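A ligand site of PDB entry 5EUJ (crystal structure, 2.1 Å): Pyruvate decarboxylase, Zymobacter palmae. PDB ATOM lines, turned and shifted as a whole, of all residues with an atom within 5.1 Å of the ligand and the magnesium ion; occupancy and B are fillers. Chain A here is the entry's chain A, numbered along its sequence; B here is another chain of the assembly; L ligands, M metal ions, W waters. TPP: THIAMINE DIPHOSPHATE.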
ATOM      1  N   GLU A 382      18.285 -24.605 -11.653  1.00  0.00           N
ATOM      2  CA  GLU A 382      17.345 -23.891 -10.786  1.00  0.00           C
ATOM      3  C   GLU A 382      16.164 -23.321 -11.547  1.00  0.00           C
ATOM      4  O   GLU A 382      16.277 -22.998 -12.735  1.00  0.00           O
ATOM      5  CB  GLU A 382      18.113 -22.775 -10.080  1.00  0.00           C
ATOM      6  CG  GLU A 382      17.340 -21.950  -9.051  1.00  0.00           C
ATOM      7  CD  GLU A 382      16.714 -22.764  -7.948  1.00  0.00           C
ATOM      8  OE1 GLU A 382      15.613 -23.287  -8.175  1.00  0.00           O
ATOM      9  OE2 GLU A 382      17.319 -22.875  -6.854  1.00  0.00           O
ATOM     10  N   THR A 383      15.023 -23.197 -10.864  1.00  0.00           N
ATOM     11  CA  THR A 383      13.883 -22.389 -11.340  1.00  0.00           C
ATOM     12  C   THR A 383      14.362 -20.966 -11.673  1.00  0.00           C
ATOM     13  O   THR A 383      15.046 -20.339 -10.882  1.00  0.00           O
ATOM     14  CB  THR A 383      12.765 -22.330 -10.280  1.00  0.00           C
ATOM     15  OG1 THR A 383      12.285 -23.659  -9.999  1.00  0.00           O
ATOM     16  CG2 THR A 383      11.597 -21.480 -10.752  1.00  0.00           C
ATOM     17  N   GLY A 384      13.997 -20.482 -12.857  1.00  0.00           N
ATOM     18  CA  GLY A 384      14.580 -19.266 -13.423  1.00  0.00           C
ATOM     19  C   GLY A 384      14.823 -19.467 -14.904  1.00  0.00           C
ATOM     20  O   GLY A 384      14.337 -20.444 -15.485  1.00  0.00           O
ATOM     21  N   ASP A 385      15.589 -18.578 -15.521  1.00  0.00           N
ATOM     22  CA  ASP A 385      15.960 -18.734 -16.937  1.00  0.00           C
ATOM     23  C   ASP A 385      16.843 -19.971 -17.179  1.00  0.00           C
ATOM     24  O   ASP A 385      16.927 -20.441 -18.310  1.00  0.00           O
ATOM     25  CB  ASP A 385      16.672 -17.476 -17.460  1.00  0.00           C
ATOM     26  CG  ASP A 385      16.671 -17.386 -18.986  1.00  0.00           C
ATOM     27  OD1 ASP A 385      15.714 -17.844 -19.646  1.00  0.00           O
ATOM     28  OD2 ASP A 385      17.632 -16.826 -19.541  1.00  0.00           O
ATOM     29  N   SER A 386      17.487 -20.477 -16.114  1.00  0.00           N
ATOM     30  CA  SER A 386      18.177 -21.771 -16.131  1.00  0.00           C
ATOM     31  C   SER A 386      17.334 -22.962 -16.604  1.00  0.00           C
ATOM     32  O   SER A 386      17.885 -23.921 -17.153  1.00  0.00           O
ATOM     33  CB  SER A 386      18.729 -22.076 -14.743  1.00  0.00           C
ATOM     34  OG  SER A 386      19.821 -21.238 -14.415  1.00  0.00           O
ATOM     35  N   GLY A 408       9.037 -26.053  -7.765  1.00  0.00           N
ATOM     36  CA  GLY A 408       9.562 -24.778  -8.234  1.00  0.00           C
ATOM     37  C   GLY A 408       9.955 -23.789  -7.153  1.00  0.00           C
ATOM     38  O   GLY A 408       9.693 -22.600  -7.284  1.00  0.00           O
ATOM     39  N   HIS A 409      10.571 -24.282  -6.089  1.00  0.00           N
ATOM     40  CA  HIS A 409      10.997 -23.467  -4.957  1.00  0.00           C
ATOM     41  C   HIS A 409      12.378 -22.887  -5.258  1.00  0.00           C
ATOM     42  O   HIS A 409      13.359 -23.624  -5.297  1.00  0.00           O
ATOM     43  CB  HIS A 409      11.046 -24.331  -3.716  1.00  0.00           C
ATOM     44  CG  HIS A 409      11.377 -23.595  -2.449  1.00  0.00           C
ATOM     45  ND1 HIS A 409      12.593 -22.981  -2.228  1.00  0.00           N
ATOM     46  CD2 HIS A 409      10.658 -23.434  -1.316  1.00  0.00           C
ATOM     47  CE1 HIS A 409      12.589 -22.450  -1.015  1.00  0.00           C
ATOM     48  NE2 HIS A 409      11.432 -22.711  -0.439  1.00  0.00           N
ATOM     49  N   ILE A 410      12.463 -21.581  -5.458  1.00  0.00           N
ATOM     50  CA  ILE A 410      13.766 -20.973  -5.779  1.00  0.00           C
ATOM     51  C   ILE A 410      14.700 -21.121  -4.590  1.00  0.00           C
ATOM     52  O   ILE A 410      14.270 -21.050  -3.443  1.00  0.00           O
ATOM     53  CB  ILE A 410      13.682 -19.513  -6.270  1.00  0.00           C
ATOM     54  CG1 ILE A 410      12.961 -18.585  -5.280  1.00  0.00           C
ATOM     55  CG2 ILE A 410      13.015 -19.481  -7.640  1.00  0.00           C
ATOM     56  CD1 ILE A 410      13.326 -17.139  -5.476  1.00  0.00           C
ATOM     57  N   GLY A 434      20.315 -18.843 -10.387  1.00  0.00           N
ATOM     58  CA  GLY A 434      20.195 -17.399 -10.557  1.00  0.00           C
ATOM     59  C   GLY A 434      20.584 -16.672  -9.287  1.00  0.00           C
ATOM     60  O   GLY A 434      20.726 -17.279  -8.228  1.00  0.00           O
ATOM     61  N   ASP A 435      20.752 -15.364  -9.412  1.00  0.00           N
ATOM     62  CA  ASP A 435      21.117 -14.529  -8.268  1.00  0.00           C
ATOM     63  C   ASP A 435      19.998 -14.494  -7.203  1.00  0.00           C
ATOM     64  O   ASP A 435      20.278 -14.610  -6.014  1.00  0.00           O
ATOM     65  CB  ASP A 435      21.556 -13.115  -8.711  1.00  0.00           C
ATOM     66  CG  ASP A 435      20.503 -12.373  -9.542  1.00  0.00           C
ATOM     67  OD1 ASP A 435      19.778 -12.982 -10.353  1.00  0.00           O
ATOM     68  OD2 ASP A 435      20.424 -11.135  -9.407  1.00  0.00           O
ATOM     69  N   GLY A 436      18.756 -14.382  -7.640  1.00  0.00           N
ATOM     70  CA  GLY A 436      17.613 -14.356  -6.733  1.00  0.00           C
ATOM     71  C   GLY A 436      17.484 -15.637  -5.923  1.00  0.00           C
ATOM     72  O   GLY A 436      17.439 -15.610  -4.692  1.00  0.00           O
ATOM     73  N   SER A 437      17.444 -16.760  -6.645  1.00  0.00           N
ATOM     74  CA  SER A 437      17.412 -18.088  -6.031  1.00  0.00           C
ATOM     75  C   SER A 437      18.508 -18.283  -5.026  1.00  0.00           C
ATOM     76  O   SER A 437      18.275 -18.726  -3.900  1.00  0.00           O
ATOM     77  CB  SER A 437      17.531 -19.158  -7.104  1.00  0.00           C
ATOM     78  OG  SER A 437      16.417 -19.126  -7.976  1.00  0.00           O
ATOM     79  N   PHE A 438      19.729 -17.951  -5.443  1.00  0.00           N
ATOM     80  CA  PHE A 438      20.915 -18.145  -4.618  1.00  0.00           C
ATOM     81  C   PHE A 438      20.792 -17.492  -3.240  1.00  0.00           C
ATOM     82  O   PHE A 438      21.229 -18.066  -2.238  1.00  0.00           O
ATOM     83  CB  PHE A 438      22.159 -17.629  -5.339  1.00  0.00           C
ATOM     84  CG  PHE A 438      23.446 -17.997  -4.648  1.00  0.00           C
ATOM     85  CD1 PHE A 438      23.986 -19.277  -4.797  1.00  0.00           C
ATOM     86  CD2 PHE A 438      24.099 -17.082  -3.849  1.00  0.00           C
ATOM     87  CE1 PHE A 438      25.162 -19.625  -4.151  1.00  0.00           C
ATOM     88  CE2 PHE A 438      25.271 -17.418  -3.200  1.00  0.00           C
ATOM     89  CZ  PHE A 438      25.810 -18.692  -3.341  1.00  0.00           C
ATOM     90  N   LEU A 440      18.199 -17.106  -1.301  1.00  0.00           N
ATOM     91  CA  LEU A 440      17.384 -17.865  -0.341  1.00  0.00           C
ATOM     92  C   LEU A 440      18.171 -18.896   0.457  1.00  0.00           C
ATOM     93  O   LEU A 440      17.865 -19.122   1.631  1.00  0.00           O
ATOM     94  CB  LEU A 440      16.206 -18.583  -1.022  1.00  0.00           C
ATOM     95  CG  LEU A 440      14.978 -17.728  -1.326  1.00  0.00           C
ATOM     96  CD1 LEU A 440      15.063 -17.123  -2.710  1.00  0.00           C
ATOM     97  CD2 LEU A 440      13.699 -18.541  -1.166  1.00  0.00           C
ATOM     98  N   ILE A 460      24.158 -17.038 -12.253  1.00  0.00           N
ATOM     99  CA  ILE A 460      23.767 -16.050 -13.271  1.00  0.00           C
ATOM    100  C   ILE A 460      23.392 -14.764 -12.548  1.00  0.00           C
ATOM    101  O   ILE A 460      22.301 -14.654 -11.969  1.00  0.00           O
ATOM    102  CB  ILE A 460      22.575 -16.518 -14.148  1.00  0.00           C
ATOM    103  CG1 ILE A 460      22.967 -17.724 -15.008  1.00  0.00           C
ATOM    104  CG2 ILE A 460      22.081 -15.384 -15.051  1.00  0.00           C
ATOM    105  CD1 ILE A 460      22.771 -19.065 -14.341  1.00  0.00           C
ATOM    106  N   ASN A 462      22.109 -11.568 -13.143  1.00  0.00           N
ATOM    107  CA  ASN A 462      21.389 -10.670 -14.034  1.00  0.00           C
ATOM    108  C   ASN A 462      20.591  -9.591 -13.293  1.00  0.00           C
ATOM    109  O   ASN A 462      19.695  -8.979 -13.862  1.00  0.00           O
ATOM    110  CB  ASN A 462      20.497 -11.473 -15.011  1.00  0.00           C
ATOM    111  CG  ASN A 462      19.493 -12.365 -14.299  1.00  0.00           C
ATOM    112  OD1 ASN A 462      19.304 -12.284 -13.080  1.00  0.00           O
ATOM    113  ND2 ASN A 462      18.837 -13.241 -15.063  1.00  0.00           N
ATOM    114  N   ARG A 463      20.918  -9.375 -12.016  1.00  0.00           N
ATOM    115  CA  ARG A 463      20.395  -8.242 -11.239  1.00  0.00           C
ATOM    116  C   ARG A 463      18.862  -8.289 -11.130  1.00  0.00           C
ATOM    117  O   ARG A 463      18.160  -7.323 -11.467  1.00  0.00           O
ATOM    118  CB  ARG A 463      20.872  -6.911 -11.851  1.00  0.00           C
ATOM    119  CG  ARG A 463      22.391  -6.800 -12.042  1.00  0.00           C
ATOM    120  CD  ARG A 463      23.135  -6.901 -10.723  1.00  0.00           C
ATOM    121  NE  ARG A 463      22.565  -5.973  -9.742  1.00  0.00           N
ATOM    122  CZ  ARG A 463      22.866  -4.666  -9.636  1.00  0.00           C
ATOM    123  NH1 ARG A 463      23.784  -4.086 -10.420  1.00  0.00           N
ATOM    124  NH2 ARG A 463      22.251  -3.931  -8.703  1.00  0.00           N
ATOM    125  N   GLY A 464      18.333  -9.434 -10.701  1.00  0.00           N
ATOM    126  CA  GLY A 464      16.906  -9.573 -10.464  1.00  0.00           C
ATOM    127  C   GLY A 464      16.262 -10.898 -10.799  1.00  0.00           C
ATOM    128  O   GLY A 464      16.908 -11.852 -11.261  1.00  0.00           O
ATOM    129  N   TYR A 465      14.959 -10.938 -10.546  1.00  0.00           N
ATOM    130  CA  TYR A 465      14.119 -12.079 -10.796  1.00  0.00           C
ATOM    131  C   TYR A 465      13.614 -11.984 -12.241  1.00  0.00           C
ATOM    132  O   TYR A 465      12.501 -11.527 -12.486  1.00  0.00           O
ATOM    133  CB  TYR A 465      12.909 -12.035  -9.839  1.00  0.00           C
ATOM    134  CG  TYR A 465      13.161 -12.161  -8.343  1.00  0.00           C
ATOM    135  CD1 TYR A 465      14.235 -12.874  -7.808  1.00  0.00           C
ATOM    136  CD2 TYR A 465      12.241 -11.617  -7.430  1.00  0.00           C
ATOM    137  CE1 TYR A 465      14.403 -13.010  -6.430  1.00  0.00           C
ATOM    138  CE2 TYR A 465      12.393 -11.748  -6.070  1.00  0.00           C
ATOM    139  CZ  TYR A 465      13.468 -12.440  -5.562  1.00  0.00           C
ATOM    140  OH  TYR A 465      13.592 -12.552  -4.195  1.00  0.00           O
ATOM    141  N   VAL A 466      14.440 -12.416 -13.197  1.00  0.00           N
ATOM    142  CA  VAL A 466      14.153 -12.190 -14.644  1.00  0.00           C
ATOM    143  C   VAL A 466      12.929 -12.941 -15.164  1.00  0.00           C
ATOM    144  O   VAL A 466      12.181 -12.404 -15.962  1.00  0.00           O
ATOM    145  CB  VAL A 466      15.414 -12.445 -15.523  1.00  0.00           C
ATOM    146  CG1 VAL A 466      15.085 -12.528 -17.013  1.00  0.00           C
ATOM    147  CG2 VAL A 466      16.410 -11.318 -15.285  1.00  0.00           C
ATOM    148  N   ILE A 467      12.751 -14.174 -14.738  1.00  0.00           N
ATOM    149  CA  ILE A 467      11.542 -14.940 -15.074  1.00  0.00           C
ATOM    150  C   ILE A 467      10.239 -14.276 -14.553  1.00  0.00           C
ATOM    151  O   ILE A 467       9.212 -14.326 -15.234  1.00  0.00           O
ATOM    152  CB  ILE A 467      11.652 -16.416 -14.603  1.00  0.00           C
ATOM    153  CG1 ILE A 467      10.421 -17.240 -14.965  1.00  0.00           C
ATOM    154  CG2 ILE A 467      11.840 -16.491 -13.105  1.00  0.00           C
ATOM    155  CD1 ILE A 467      10.690 -18.731 -15.006  1.00  0.00           C
ATOM    156  N   GLU A 468      10.299 -13.668 -13.369  1.00  0.00           N
ATOM    157  CA  GLU A 468       9.156 -12.893 -12.859  1.00  0.00           C
ATOM    158  C   GLU A 468       8.920 -11.618 -13.654  1.00  0.00           C
ATOM    159  O   GLU A 468       7.782 -11.219 -13.852  1.00  0.00           O
ATOM    160  CB  GLU A 468       9.317 -12.535 -11.377  1.00  0.00           C
ATOM    161  CG  GLU A 468       9.282 -13.721 -10.433  1.00  0.00           C
ATOM    162  CD  GLU A 468       7.917 -14.407 -10.387  1.00  0.00           C
ATOM    163  OE1 GLU A 468       6.987 -13.857  -9.760  1.00  0.00           O
ATOM    164  OE2 GLU A 468       7.786 -15.487 -10.995  1.00  0.00           O
ATOM    165  N   VAL B  23       7.679 -11.372  -0.378  1.00  0.00           N
ATOM    166  CA  VAL B  23       8.521 -12.063  -1.364  1.00  0.00           C
ATOM    167  C   VAL B  23       7.623 -12.353  -2.567  1.00  0.00           C
ATOM    168  O   VAL B  23       6.609 -13.025  -2.445  1.00  0.00           O
ATOM    169  CB  VAL B  23       9.104 -13.373  -0.802  1.00  0.00           C
ATOM    170  CG1 VAL B  23      10.018 -14.040  -1.839  1.00  0.00           C
ATOM    171  CG2 VAL B  23       9.872 -13.093   0.471  1.00  0.00           C
ATOM    172  N   ALA B  24       7.993 -11.828  -3.725  1.00  0.00           N
ATOM    173  CA  ALA B  24       7.161 -11.956  -4.917  1.00  0.00           C
ATOM    174  C   ALA B  24       7.083 -13.402  -5.402  1.00  0.00           C
ATOM    175  O   ALA B  24       7.976 -14.188  -5.130  1.00  0.00           O
ATOM    176  CB  ALA B  24       7.668 -11.068  -6.042  1.00  0.00           C
ATOM    177  N   GLY B  25       5.982 -13.701  -6.098  1.00  0.00           N
ATOM    178  CA  GLY B  25       5.808 -14.946  -6.822  1.00  0.00           C
ATOM    179  C   GLY B  25       4.579 -14.766  -7.693  1.00  0.00           C
ATOM    180  O   GLY B  25       3.726 -13.951  -7.368  1.00  0.00           O
ATOM    181  N   ASP B  26       4.477 -15.511  -8.780  1.00  0.00           N
ATOM    182  CA  ASP B  26       3.422 -15.226  -9.765  1.00  0.00           C
ATOM    183  C   ASP B  26       1.980 -15.248  -9.206  1.00  0.00           C
ATOM    184  O   ASP B  26       1.121 -14.554  -9.727  1.00  0.00           O
ATOM    185  CB  ASP B  26       3.583 -16.034 -11.070  1.00  0.00           C
ATOM    186  CG  ASP B  26       3.387 -17.554 -10.903  1.00  0.00           C
ATOM    187  OD1 ASP B  26       3.419 -18.082  -9.758  1.00  0.00           O
ATOM    188  OD2 ASP B  26       3.216 -18.206 -11.967  1.00  0.00           O
ATOM    189  N   GLU B  49      11.171 -16.463   2.614  1.00  0.00           N
ATOM    190  CA  GLU B  49       9.876 -16.315   3.267  1.00  0.00           C
ATOM    191  C   GLU B  49       9.939 -16.591   4.758  1.00  0.00           C
ATOM    192  O   GLU B  49       9.164 -15.991   5.511  1.00  0.00           O
ATOM    193  CB  GLU B  49       8.821 -17.201   2.587  1.00  0.00           C
ATOM    194  CG  GLU B  49       8.491 -16.758   1.168  1.00  0.00           C
ATOM    195  CD  GLU B  49       9.379 -17.398   0.095  1.00  0.00           C
ATOM    196  OE1 GLU B  49      10.425 -17.988   0.420  1.00  0.00           O
ATOM    197  OE2 GLU B  49       9.002 -17.306  -1.082  1.00  0.00           O
ATOM    198  N   THR B  71       3.939 -16.235  -1.706  1.00  0.00           N
ATOM    199  CA  THR B  71       3.310 -16.992  -2.791  1.00  0.00           C
ATOM    200  C   THR B  71       2.897 -18.371  -2.281  1.00  0.00           C
ATOM    201  O   THR B  71       3.341 -18.815  -1.220  1.00  0.00           O
ATOM    202  CB  THR B  71       4.228 -17.086  -4.033  1.00  0.00           C
ATOM    203  OG1 THR B  71       3.457 -17.455  -5.173  1.00  0.00           O
ATOM    204  CG2 THR B  71       5.357 -18.101  -3.858  1.00  0.00           C
ATOM    205  N   VAL B  74       5.285 -22.825  -1.851  1.00  0.00           N
ATOM    206  CA  VAL B  74       6.739 -22.650  -1.792  1.00  0.00           C
ATOM    207  C   VAL B  74       7.112 -21.518  -0.847  1.00  0.00           C
ATOM    208  O   VAL B  74       8.094 -21.630  -0.102  1.00  0.00           O
ATOM    209  CB  VAL B  74       7.386 -22.465  -3.185  1.00  0.00           C
ATOM    210  CG1 VAL B  74       7.356 -23.779  -3.934  1.00  0.00           C
ATOM    211  CG2 VAL B  74       6.732 -21.365  -3.995  1.00  0.00           C
ATOM    212  N   GLY B  75       6.299 -20.451  -0.820  1.00  0.00           N
ATOM    213  CA  GLY B  75       6.491 -19.376   0.131  1.00  0.00           C
ATOM    214  C   GLY B  75       5.857 -19.661   1.472  1.00  0.00           C
ATOM    215  O   GLY B  75       6.524 -19.727   2.499  1.00  0.00           O
ATOM    216  N   HIS B 113       3.846 -25.125  -7.997  1.00  0.00           N
ATOM    217  CA  HIS B 113       3.981 -24.925  -6.548  1.00  0.00           C
ATOM    218  C   HIS B 113       2.965 -25.706  -5.718  1.00  0.00           C
ATOM    219  O   HIS B 113       2.627 -25.269  -4.644  1.00  0.00           O
ATOM    220  CB  HIS B 113       3.868 -23.426  -6.119  1.00  0.00           C
ATOM    221  CG  HIS B 113       4.793 -22.500  -6.843  1.00  0.00           C
ATOM    222  ND1 HIS B 113       6.049 -22.873  -7.288  1.00  0.00           N
ATOM    223  CD2 HIS B 113       4.678 -21.182  -7.146  1.00  0.00           C
ATOM    224  CE1 HIS B 113       6.634 -21.848  -7.858  1.00  0.00           C
ATOM    225  NE2 HIS B 113       5.825 -20.805  -7.777  1.00  0.00           N
HETATM  226  N1' TPP L   1       9.674 -17.894  -3.594  1.00  0.00           N
HETATM  227  C2' TPP L   1       9.935 -19.233  -3.642  1.00  0.00           C
HETATM  228  CM2 TPP L   1      10.406 -19.939  -2.410  1.00  0.00           C
HETATM  229  N3' TPP L   1       9.806 -19.929  -4.791  1.00  0.00           N
HETATM  230  C4' TPP L   1       9.390 -19.307  -5.919  1.00  0.00           C
HETATM  231  N4' TPP L   1       9.247 -20.038  -7.035  1.00  0.00           N
HETATM  232  C5' TPP L   1       9.080 -17.847  -5.876  1.00  0.00           C
HETATM  233  C6' TPP L   1       9.247 -17.203  -4.661  1.00  0.00           C
HETATM  234  C7' TPP L   1       8.618 -17.089  -7.117  1.00  0.00           C
HETATM  235  N3  TPP L   1       9.692 -16.974  -8.132  1.00  0.00           N
HETATM  236  C2  TPP L   1       9.814 -17.832  -9.177  1.00  0.00           C
HETATM  237  S1  TPP L   1      11.131 -17.628 -10.320  1.00  0.00           S
HETATM  238  C5  TPP L   1      11.574 -16.260  -9.341  1.00  0.00           C
HETATM  239  C4  TPP L   1      10.669 -16.031  -8.176  1.00  0.00           C
HETATM  240  CM4 TPP L   1      10.877 -14.888  -7.218  1.00  0.00           C
HETATM  241  C6  TPP L   1      12.777 -15.504  -9.828  1.00  0.00           C
HETATM  242  C7  TPP L   1      14.066 -16.321  -9.833  1.00  0.00           C
HETATM  243  O7  TPP L   1      15.132 -15.379  -9.970  1.00  0.00           O
HETATM  244  PA  TPP L   1      16.620 -15.838 -10.305  1.00  0.00           P
HETATM  245  O1A TPP L   1      17.028 -16.914  -9.359  1.00  0.00           O
HETATM  246  O2A TPP L   1      17.479 -14.615 -10.278  1.00  0.00           O
HETATM  247  O3A TPP L   1      16.398 -16.419 -11.792  1.00  0.00           O
HETATM  248  PB  TPP L   1      16.333 -15.609 -13.183  1.00  0.00           P
HETATM  249  O1B TPP L   1      14.912 -15.652 -13.655  1.00  0.00           O
HETATM  250  O2B TPP L   1      17.300 -16.393 -14.071  1.00  0.00           O
HETATM  251  O3B TPP L   1      16.805 -14.202 -12.932  1.00  0.00           O
HETATM  252 MG    MG M   1      18.203 -13.438 -11.622  1.00  0.00          MG
HETATM  253  O   HOH W   1      17.535 -19.286 -10.885  1.00  0.00           O
HETATM  254  O   HOH W   2      18.595 -19.092 -13.592  1.00  0.00           O
HETATM  255  O   HOH W   3       6.709 -17.808 -10.022  1.00  0.00           O
HETATM  256  O   HOH W   4      19.557 -14.994 -12.444  1.00  0.00           O
HETATM  257  O   HOH W   5       8.364 -19.478 -11.521  1.00  0.00           O
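CG2 of Thr 383 touches S1 of the ligand, at 3.9 Å. Gly 384 touches the ligand (CA to O1B, 3.6 Å). His 409 touches the ligand (NE2 to CM2, 3.6 Å). Gly 434 touches the ligand. Leu 440 touches the ligand (CD2 to CM2, 3.8 Å). CD1 of Tyr 465 touches O7 of the ligand, 3.4 Å away. Glu 468 touches the ligand (CG to C4, 3.5 Å). Ala 24 of chain B touches the ligand (O to C6', 3.3 Å). Gly 25 of chain B touches the ligand. Val 74 of chain B touches the ligand (CG2 to N3', 3.5 Å). His 113 of chain B touches the ligand. Of the 31 residues printed, 22 come within 4 Å of the ligand. Along chain A the residues within 4 Å of the ligand span positions 383 to 468.
The magnesium ion is bound by an oxygen (O2A) of the ligand (1.9 Å), an oxygen (O3B) of the ligand (2.1 Å), the side-chain carboxylate (OD1) of Asp 435 (2.1 Å), the backbone carbonyl oxygen (O) of Gly 464 (2.1 Å), the side-chain amide oxygen (OD1) of Asn 462 (2.2 Å) and water W4 (2.2 Å).
The nearest printed residue that does not touch the magnesium ion is Gly 436 (4.1 Å).
The backbone NH (N) of Asp 435 sits close to an oxygen (O2A) of the ligand, 3.5 Å away. N4' of the ligand is in hydrogen-bond range of O of Gly 408. OE2 of Glu 49 of chain B sits at hydrogen-bond distance from N1' of the ligand, 2.7 Å away. O1A of the ligand is in hydrogen-bond range of N of Ser 437, at 2.8 Å. The side-chain hydroxyl of Ser 437 lies within hydrogen-bond range of an oxygen (O1A) of the ligand, 2.7 Å away. An oxygen (O1B) of the ligand sits at hydrogen-bond distance from the backbone NH (N) of Ile 467, at 2.8 Å. N of Gly 436 sits close to O2A of the ligand (2.9 Å). The backbone NH of Val 466 is in hydrogen-bond range of an oxygen (O1B) of the ligand (3.3 Å). The backbone NH (N) of Asp 385 lies within hydrogen-bond range of an oxygen (O2B) of the ligand. N of Ile 410 sits at hydrogen-bond distance from N3' of the ligand.
The backbone carbonyl oxygen of Ile 460 is in hydrogen-bond range of the backbone NH of Asp 435. OD2 of Asp 435 sits at hydrogen-bond distance from N of Arg 463 (3.2 Å). The backbone carbonyl oxygen of Thr 383 sits at hydrogen-bond distance from the side-chain hydroxyl of Ser 437 (3.4 Å). OE1 of Glu 468 lies within hydrogen-bond range of N of Asp 26 of chain B.
Water W4 lies within hydrogen-bond range of O of Ile 460, O2B of the ligand, ND2 of Asn 462 and N of Asp 435. Water W1 lies within hydrogen-bond range of O of Thr 383 (2.7 Å), N of Gly 434 (2.9 Å), O1A of the ligand (2.9 Å) and OG of Ser 437 (3.1 Å). Water W2 bridges OG of Ser 386 (2.6 Å) and O2B of the ligand (3.0 Å). Water W3 lies within hydrogen-bond range of OE2 of Glu 468 and OD1 of Asp 26 of chain B.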
